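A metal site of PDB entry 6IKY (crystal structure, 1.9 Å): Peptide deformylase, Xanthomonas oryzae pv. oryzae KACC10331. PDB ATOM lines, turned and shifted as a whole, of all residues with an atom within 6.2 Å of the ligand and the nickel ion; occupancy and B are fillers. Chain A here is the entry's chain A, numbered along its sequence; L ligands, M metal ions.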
ATOM      1  N   MET A  39     -18.206  22.573  14.208  1.00  0.00           N
ATOM      2  CA  MET A  39     -18.868  23.634  14.976  1.00  0.00           C
ATOM      3  C   MET A  39     -18.079  24.978  14.887  1.00  0.00           C
ATOM      4  O   MET A  39     -18.676  26.027  14.693  1.00  0.00           O
ATOM      5  CB  MET A  39     -19.050  23.198  16.430  1.00  0.00           C
ATOM      6  CG  MET A  39     -19.770  24.203  17.302  1.00  0.00           C
ATOM      7  SD  MET A  39     -20.142  23.677  18.979  1.00  0.00           S
ATOM      8  CE  MET A  39     -18.758  24.161  19.958  1.00  0.00           C
ATOM      9  N   ALA A  42     -18.273  26.671  11.386  1.00  0.00           N
ATOM     10  CA  ALA A  42     -19.583  27.236  11.204  1.00  0.00           C
ATOM     11  C   ALA A  42     -19.849  28.371  12.216  1.00  0.00           C
ATOM     12  O   ALA A  42     -20.921  28.915  12.160  1.00  0.00           O
ATOM     13  CB  ALA A  42     -20.631  26.141  11.375  1.00  0.00           C
ATOM     14  N   HIS A  43     -18.955  28.652  13.147  1.00  0.00           N
ATOM     15  CA  HIS A  43     -19.172  29.662  14.190  1.00  0.00           C
ATOM     16  C   HIS A  43     -20.410  29.335  15.051  1.00  0.00           C
ATOM     17  O   HIS A  43     -21.148  30.201  15.503  1.00  0.00           O
ATOM     18  CB  HIS A  43     -19.242  31.087  13.613  1.00  0.00           C
ATOM     19  CG  HIS A  43     -18.008  31.538  12.859  1.00  0.00           C
ATOM     20  ND1 HIS A  43     -17.796  32.862  12.564  1.00  0.00           N
ATOM     21  CD2 HIS A  43     -16.952  30.870  12.320  1.00  0.00           C
ATOM     22  CE1 HIS A  43     -16.678  32.992  11.874  1.00  0.00           C
ATOM     23  NE2 HIS A  43     -16.108  31.813  11.753  1.00  0.00           N
ATOM     24  N   GLY A  44     -20.602  28.060  15.357  1.00  0.00           N
ATOM     25  CA  GLY A  44     -21.661  27.652  16.297  1.00  0.00           C
ATOM     26  C   GLY A  44     -21.274  27.657  17.757  1.00  0.00           C
ATOM     27  O   GLY A  44     -20.101  27.714  18.049  1.00  0.00           O
ATOM     28  N   VAL A  45     -22.264  27.639  18.667  1.00  0.00           N
ATOM     29  CA  VAL A  45     -22.054  27.335  20.086  1.00  0.00           C
ATOM     30  C   VAL A  45     -22.523  25.901  20.494  1.00  0.00           C
ATOM     31  O   VAL A  45     -22.416  25.476  21.656  1.00  0.00           O
ATOM     32  CB  VAL A  45     -22.701  28.400  21.006  1.00  0.00           C
ATOM     33  CG1 VAL A  45     -22.072  29.777  20.726  1.00  0.00           C
ATOM     34  CG2 VAL A  45     -24.190  28.388  20.829  1.00  0.00           C
ATOM     35  N   GLY A  46     -23.106  25.182  19.559  1.00  0.00           N
ATOM     36  CA  GLY A  46     -23.563  23.838  19.820  1.00  0.00           C
ATOM     37  C   GLY A  46     -23.642  23.155  18.477  1.00  0.00           C
ATOM     38  O   GLY A  46     -23.770  23.830  17.448  1.00  0.00           O
ATOM     39  N   LEU A  47     -23.577  21.846  18.465  1.00  0.00           N
ATOM     40  CA  LEU A  47     -23.795  21.062  17.257  1.00  0.00           C
ATOM     41  C   LEU A  47     -24.214  19.640  17.666  1.00  0.00           C
ATOM     42  O   LEU A  47     -23.545  19.002  18.515  1.00  0.00           O
ATOM     43  CB  LEU A  47     -22.501  21.037  16.449  1.00  0.00           C
ATOM     44  CG  LEU A  47     -22.619  20.197  15.164  1.00  0.00           C
ATOM     45  CD1 LEU A  47     -23.452  20.875  14.075  1.00  0.00           C
ATOM     46  CD2 LEU A  47     -21.258  19.802  14.599  1.00  0.00           C
ATOM     47  N   ALA A  48     -25.263  19.097  17.070  1.00  0.00           N
ATOM     48  CA  ALA A  48     -25.693  17.745  17.427  1.00  0.00           C
ATOM     49  C   ALA A  48     -25.334  16.840  16.303  1.00  0.00           C
ATOM     50  O   ALA A  48     -25.307  17.221  15.161  1.00  0.00           O
ATOM     51  CB  ALA A  48     -27.184  17.685  17.756  1.00  0.00           C
ATOM     52  N   GLN A  51     -27.126  16.769  12.923  1.00  0.00           N
ATOM     53  CA  GLN A  51     -26.866  17.827  11.963  1.00  0.00           C
ATOM     54  C   GLN A  51     -25.751  17.546  10.952  1.00  0.00           C
ATOM     55  O   GLN A  51     -25.681  18.237   9.930  1.00  0.00           O
ATOM     56  CB  GLN A  51     -26.536  19.165  12.646  1.00  0.00           C
ATOM     57  CG  GLN A  51     -27.663  19.671  13.513  1.00  0.00           C
ATOM     58  CD  GLN A  51     -27.316  20.961  14.248  1.00  0.00           C
ATOM     59  OE1 GLN A  51     -26.754  20.911  15.348  1.00  0.00           O
ATOM     60  NE2 GLN A  51     -27.636  22.124  13.638  1.00  0.00           N
ATOM     61  N   TRP A  96     -33.261  34.672  22.216  1.00  0.00           N
ATOM     62  CA  TRP A  96     -32.967  34.452  20.788  1.00  0.00           C
ATOM     63  C   TRP A  96     -32.272  33.087  20.476  1.00  0.00           C
ATOM     64  O   TRP A  96     -31.321  32.659  21.165  1.00  0.00           O
ATOM     65  CB  TRP A  96     -32.109  35.601  20.268  1.00  0.00           C
ATOM     66  CG  TRP A  96     -32.831  36.929  20.170  1.00  0.00           C
ATOM     67  CD1 TRP A  96     -32.702  38.040  20.977  1.00  0.00           C
ATOM     68  CD2 TRP A  96     -33.816  37.270  19.159  1.00  0.00           C
ATOM     69  NE1 TRP A  96     -33.573  39.047  20.523  1.00  0.00           N
ATOM     70  CE2 TRP A  96     -34.244  38.601  19.416  1.00  0.00           C
ATOM     71  CE3 TRP A  96     -34.395  36.564  18.087  1.00  0.00           C
ATOM     72  CZ2 TRP A  96     -35.236  39.244  18.608  1.00  0.00           C
ATOM     73  CZ3 TRP A  96     -35.332  37.204  17.297  1.00  0.00           C
ATOM     74  CH2 TRP A  96     -35.755  38.547  17.581  1.00  0.00           C
ATOM     75  N   GLU A  97     -32.687  32.431  19.397  1.00  0.00           N
ATOM     76  CA  GLU A  97     -31.964  31.259  18.912  1.00  0.00           C
ATOM     77  C   GLU A  97     -31.839  31.305  17.422  1.00  0.00           C
ATOM     78  O   GLU A  97     -32.733  31.846  16.716  1.00  0.00           O
ATOM     79  CB  GLU A  97     -32.665  29.933  19.284  1.00  0.00           C
ATOM     80  CG  GLU A  97     -32.849  29.794  20.797  1.00  0.00           C
ATOM     81  CD  GLU A  97     -33.385  28.438  21.315  1.00  0.00           C
ATOM     82  OE1 GLU A  97     -33.471  27.448  20.559  1.00  0.00           O
ATOM     83  OE2 GLU A  97     -33.785  28.374  22.536  1.00  0.00           O
ATOM     84  N   GLY A  98     -30.767  30.702  16.944  1.00  0.00           N
ATOM     85  CA  GLY A  98     -30.625  30.347  15.556  1.00  0.00           C
ATOM     86  C   GLY A  98     -30.131  28.896  15.520  1.00  0.00           C
ATOM     87  O   GLY A  98     -29.977  28.259  16.564  1.00  0.00           O
ATOM     88  N   CSD A  99     -29.892  28.396  14.332  1.00  0.00           N
ATOM     89  CA  CSD A  99     -29.539  27.009  14.110  1.00  0.00           C
ATOM     90  CB  CSD A  99     -30.841  26.203  14.003  1.00  0.00           C
ATOM     91  SG  CSD A  99     -30.710  24.483  14.168  1.00  0.00           S
ATOM     92  C   CSD A  99     -28.735  26.961  12.827  1.00  0.00           C
ATOM     93  O   CSD A  99     -29.106  27.565  11.828  1.00  0.00           O
ATOM     94  OD1 CSD A  99     -29.748  24.185  13.123  1.00  0.00           O
ATOM     95  OD2 CSD A  99     -31.743  23.880  13.076  1.00  0.00           O
ATOM     96  N   LEU A 100     -27.628  26.209  12.848  1.00  0.00           N
ATOM     97  CA  LEU A 100     -26.784  26.021  11.680  1.00  0.00           C
ATOM     98  C   LEU A 100     -27.469  25.269  10.539  1.00  0.00           C
ATOM     99  O   LEU A 100     -27.049  25.359   9.403  1.00  0.00           O
ATOM    100  CB  LEU A 100     -25.491  25.259  12.079  1.00  0.00           C
ATOM    101  CG  LEU A 100     -24.653  26.023  13.103  1.00  0.00           C
ATOM    102  CD1 LEU A 100     -23.658  25.101  13.828  1.00  0.00           C
ATOM    103  CD2 LEU A 100     -24.052  27.241  12.433  1.00  0.00           C
ATOM    104  N   SER A 101     -28.467  24.449  10.841  1.00  0.00           N
ATOM    105  CA  SER A 101     -29.233  23.789   9.798  1.00  0.00           C
ATOM    106  C   SER A 101     -30.357  24.727   9.232  1.00  0.00           C
ATOM    107  O   SER A 101     -31.103  24.347   8.334  1.00  0.00           O
ATOM    108  CB  SER A 101     -29.851  22.515  10.344  1.00  0.00           C
ATOM    109  OG  SER A 101     -28.832  21.587  10.799  1.00  0.00           O
ATOM    110  N   PHE A 134     -28.294  30.792  29.443  1.00  0.00           N
ATOM    111  CA  PHE A 134     -27.774  30.507  28.111  1.00  0.00           C
ATOM    112  C   PHE A 134     -27.183  29.100  28.015  1.00  0.00           C
ATOM    113  O   PHE A 134     -27.541  28.284  27.113  1.00  0.00           O
ATOM    114  CB  PHE A 134     -26.797  31.590  27.616  1.00  0.00           C
ATOM    115  CG  PHE A 134     -26.493  31.436  26.144  1.00  0.00           C
ATOM    116  CD1 PHE A 134     -27.497  31.605  25.209  1.00  0.00           C
ATOM    117  CD2 PHE A 134     -25.255  31.067  25.682  1.00  0.00           C
ATOM    118  CE1 PHE A 134     -27.260  31.435  23.846  1.00  0.00           C
ATOM    119  CE2 PHE A 134     -25.011  30.885  24.322  1.00  0.00           C
ATOM    120  CZ  PHE A 134     -26.011  31.066  23.414  1.00  0.00           C
ATOM    121  N   ARG A 137     -30.103  26.745  27.755  1.00  0.00           N
ATOM    122  CA  ARG A 137     -30.769  26.876  26.456  1.00  0.00           C
ATOM    123  C   ARG A 137     -30.074  26.101  25.360  1.00  0.00           C
ATOM    124  O   ARG A 137     -30.721  25.411  24.585  1.00  0.00           O
ATOM    125  CB  ARG A 137     -30.745  28.355  26.017  1.00  0.00           C
ATOM    126  CG  ARG A 137     -31.320  28.612  24.633  1.00  0.00           C
ATOM    127  CD  ARG A 137     -31.394  30.155  24.407  1.00  0.00           C
ATOM    128  NE  ARG A 137     -32.269  30.800  25.394  1.00  0.00           N
ATOM    129  CZ  ARG A 137     -33.608  30.899  25.349  1.00  0.00           C
ATOM    130  NH1 ARG A 137     -34.273  30.441  24.343  1.00  0.00           N
ATOM    131  NH2 ARG A 137     -34.301  31.448  26.364  1.00  0.00           N
ATOM    132  N   VAL A 138     -28.753  26.243  25.341  1.00  0.00           N
ATOM    133  CA  VAL A 138     -27.954  25.534  24.348  1.00  0.00           C
ATOM    134  C   VAL A 138     -28.176  24.059  24.459  1.00  0.00           C
ATOM    135  O   VAL A 138     -28.414  23.350  23.468  1.00  0.00           O
ATOM    136  CB  VAL A 138     -26.463  25.846  24.474  1.00  0.00           C
ATOM    137  CG1 VAL A 138     -25.672  25.031  23.417  1.00  0.00           C
ATOM    138  CG2 VAL A 138     -26.249  27.291  24.130  1.00  0.00           C
ATOM    139  N   HIS A 141     -31.585  23.069  23.237  1.00  0.00           N
ATOM    140  CA  HIS A 141     -31.675  23.184  21.767  1.00  0.00           C
ATOM    141  C   HIS A 141     -31.015  21.958  21.116  1.00  0.00           C
ATOM    142  O   HIS A 141     -31.599  21.337  20.266  1.00  0.00           O
ATOM    143  CB  HIS A 141     -30.947  24.454  21.342  1.00  0.00           C
ATOM    144  CG  HIS A 141     -30.866  24.632  19.861  1.00  0.00           C
ATOM    145  ND1 HIS A 141     -31.624  25.560  19.175  1.00  0.00           N
ATOM    146  CD2 HIS A 141     -30.123  23.972  18.933  1.00  0.00           C
ATOM    147  CE1 HIS A 141     -31.364  25.435  17.872  1.00  0.00           C
ATOM    148  NE2 HIS A 141     -30.445  24.495  17.703  1.00  0.00           N
ATOM    149  N   GLU A 142     -29.848  21.560  21.609  1.00  0.00           N
ATOM    150  CA  GLU A 142     -29.186  20.400  21.018  1.00  0.00           C
ATOM    151  C   GLU A 142     -29.895  19.110  21.311  1.00  0.00           C
ATOM    152  O   GLU A 142     -29.936  18.219  20.449  1.00  0.00           O
ATOM    153  CB  GLU A 142     -27.728  20.331  21.472  1.00  0.00           C
ATOM    154  CG  GLU A 142     -26.796  21.484  21.078  1.00  0.00           C
ATOM    155  CD  GLU A 142     -27.000  21.960  19.648  1.00  0.00           C
ATOM    156  OE1 GLU A 142     -27.162  21.137  18.694  1.00  0.00           O
ATOM    157  OE2 GLU A 142     -27.009  23.181  19.450  1.00  0.00           O
ATOM    158  N   HIS A 145     -32.502  18.256  18.889  1.00  0.00           N
ATOM    159  CA  HIS A 145     -32.049  17.565  17.634  1.00  0.00           C
ATOM    160  C   HIS A 145     -32.027  16.034  17.718  1.00  0.00           C
ATOM    161  O   HIS A 145     -32.317  15.291  16.763  1.00  0.00           O
ATOM    162  CB  HIS A 145     -30.658  18.010  17.273  1.00  0.00           C
ATOM    163  CG  HIS A 145     -30.592  19.340  16.616  1.00  0.00           C
ATOM    164  ND1 HIS A 145     -31.241  19.583  15.430  1.00  0.00           N
ATOM    165  CD2 HIS A 145     -29.983  20.500  16.973  1.00  0.00           C
ATOM    166  CE1 HIS A 145     -30.979  20.830  15.055  1.00  0.00           C
ATOM    167  NE2 HIS A 145     -30.236  21.394  15.968  1.00  0.00           N
ATOM    168  N   LEU A 150     -36.941  20.816  15.672  1.00  0.00           N
ATOM    169  CA  LEU A 150     -36.261  22.059  15.391  1.00  0.00           C
ATOM    170  C   LEU A 150     -37.010  23.229  16.008  1.00  0.00           C
ATOM    171  O   LEU A 150     -38.229  23.114  16.313  1.00  0.00           O
ATOM    172  CB  LEU A 150     -36.207  22.222  13.889  1.00  0.00           C
ATOM    173  CG  LEU A 150     -35.589  21.010  13.157  1.00  0.00           C
ATOM    174  CD1 LEU A 150     -35.884  21.098  11.682  1.00  0.00           C
ATOM    175  CD2 LEU A 150     -34.087  21.022  13.499  1.00  0.00           C
ATOM    176  N   TYR A 151     -36.319  24.340  16.169  1.00  0.00           N
ATOM    177  CA  TYR A 151     -36.869  25.421  16.953  1.00  0.00           C
ATOM    178  C   TYR A 151     -38.156  26.084  16.343  1.00  0.00           C
ATOM    179  O   TYR A 151     -38.906  26.666  17.118  1.00  0.00           O
ATOM    180  CB  TYR A 151     -35.826  26.483  17.309  1.00  0.00           C
ATOM    181  CG  TYR A 151     -35.426  27.430  16.220  1.00  0.00           C
ATOM    182  CD1 TYR A 151     -36.296  28.535  15.819  1.00  0.00           C
ATOM    183  CD2 TYR A 151     -34.212  27.332  15.598  1.00  0.00           C
ATOM    184  CE1 TYR A 151     -35.928  29.380  14.784  1.00  0.00           C
ATOM    185  CE2 TYR A 151     -33.806  28.225  14.611  1.00  0.00           C
ATOM    186  CZ  TYR A 151     -34.667  29.252  14.193  1.00  0.00           C
ATOM    187  OH  TYR A 151     -34.288  30.097  13.189  1.00  0.00           O
HETATM  188  O1  LIG L   1     -28.232  22.938  16.802  1.00  0.00           O
HETATM  189  C1  LIG L   1     -27.615  23.991  16.453  1.00  0.00           C
HETATM  190  O2  LIG L   1     -27.871  24.562  15.274  1.00  0.00           O
HETATM  191  C2  LIG L   1     -26.541  24.863  17.040  1.00  0.00           C
HETATM  192  C3  LIG L   1     -26.915  26.369  17.314  1.00  0.00           C
HETATM  193  C4  LIG L   1     -27.068  26.407  18.866  1.00  0.00           C
HETATM  194  C5  LIG L   1     -27.791  27.540  19.600  1.00  0.00           C
HETATM  195  C6  LIG L   1     -28.686  27.172  20.596  1.00  0.00           C
HETATM  196  C7  LIG L   1     -29.375  28.106  21.365  1.00  0.00           C
HETATM  197  C8  LIG L   1     -29.178  29.467  21.148  1.00  0.00           C
HETATM  198  C9  LIG L   1     -28.311  29.858  20.142  1.00  0.00           C
HETATM  199  C10 LIG L   1     -27.615  28.904  19.374  1.00  0.00           C
HETATM  200  C11 LIG L   1     -25.905  27.357  16.626  1.00  0.00           C
HETATM  201  O3  LIG L   1     -24.758  27.528  17.438  1.00  0.00           O
HETATM  202  S1  LIG L   1     -26.453  29.021  16.131  1.00  0.00           S
HETATM  203  C12 LIG L   1     -25.248  30.357  16.082  1.00  0.00           C
HETATM  204  C13 LIG L   1     -25.252  31.326  17.279  1.00  0.00           C
HETATM  205  C14 LIG L   1     -26.445  31.826  17.863  1.00  0.00           C
HETATM  206  C15 LIG L   1     -26.383  32.700  18.975  1.00  0.00           C
HETATM  207  C16 LIG L   1     -25.152  33.094  19.531  1.00  0.00           C
HETATM  208  C17 LIG L   1     -23.967  32.610  18.960  1.00  0.00           C
HETATM  209  C18 LIG L   1     -24.023  31.735  17.855  1.00  0.00           C
HETATM  210 NI    NI M   1     -29.626  23.627  15.870  1.00  0.00          NI
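An oxygen (O3) of the ligand lies within hydrogen-bond range of the backbone NH (N) of Val 45, at 2.8 Å.
The side-chain amide oxygen (OE1) of Gln 51 lies close to an oxygen (O1) of the ligand (2.9 Å).
The backbone NH (N) of Leu 100 lies close to an oxygen (O2) of the ligand (2.9 Å).
OE1 of Gln 51 sits close to OE1 of Glu 142, at 3.4 Å.
The backbone NH (N) of Gly 44 sits at hydrogen-bond distance from the backbone carbonyl oxygen (O) of Met 39.
N of Ala 48 is in hydrogen-bond range of OE1 of Gln 51 (2.9 Å).
The side-chain carboxylate (OE1) of Glu 142 sits at hydrogen-bond distance from the backbone NH (N) of Ala 48 (3.2 Å).
NE2 of Gln 51 is in hydrogen-bond range of OG of Ser 101 (3.1 Å).
OD1 of CSD 99 lies within hydrogen-bond range of NE2 of Gln 51, 3.0 Å away.
ND1 of His 141 sits at hydrogen-bond distance from OE1 of Glu 97 (3.0 Å).
The guanidinium group (NH1) of Arg 137 is in salt-bridge range of the side-chain carboxylate (OE2) of Glu 97.
O of Gly 98 lies close to S1 of the ligand, at 3.6 Å.
The side-chain carboxylate (OE1) of Glu 142 sits close to an oxygen (O1) of the ligand, 2.8 Å away.
Merely in contact with the ligand: Gly 46 (3.0 Å), Gly 44 (3.3 Å), Glu 97 (3.7 Å), Arg 137 (3.8 Å), Trp 96 (3.8 Å) and Phe 134 (3.9 Å).
Hydrophobic or aromatic side chains within 4 Å of the ligand: Val 45, Leu 100, Phe 134, His 141 and His 145.
Gln 51 touches the nickel ion (NE2 to NI, 3.3 Å).
Four residues have an atom within 4 Å of the nickel ion: Gln 51, CSD 99, His 141 and His 145.
The nearest printed residue that does not touch the nickel ion is Leu 100 (4.4 Å).
An oxygen (O1) of the ligand is bound to the nickel ion (1.8 Å).
The nickel ion is bound by O2 of the ligand.
The nickel ion is bound by NE2 of His 141.
SG of CSD 99 is bound to the nickel ion (2.2 Å).
The nickel ion is bound by a ring nitrogen (NE2) of His 145, at 2.3 Å.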
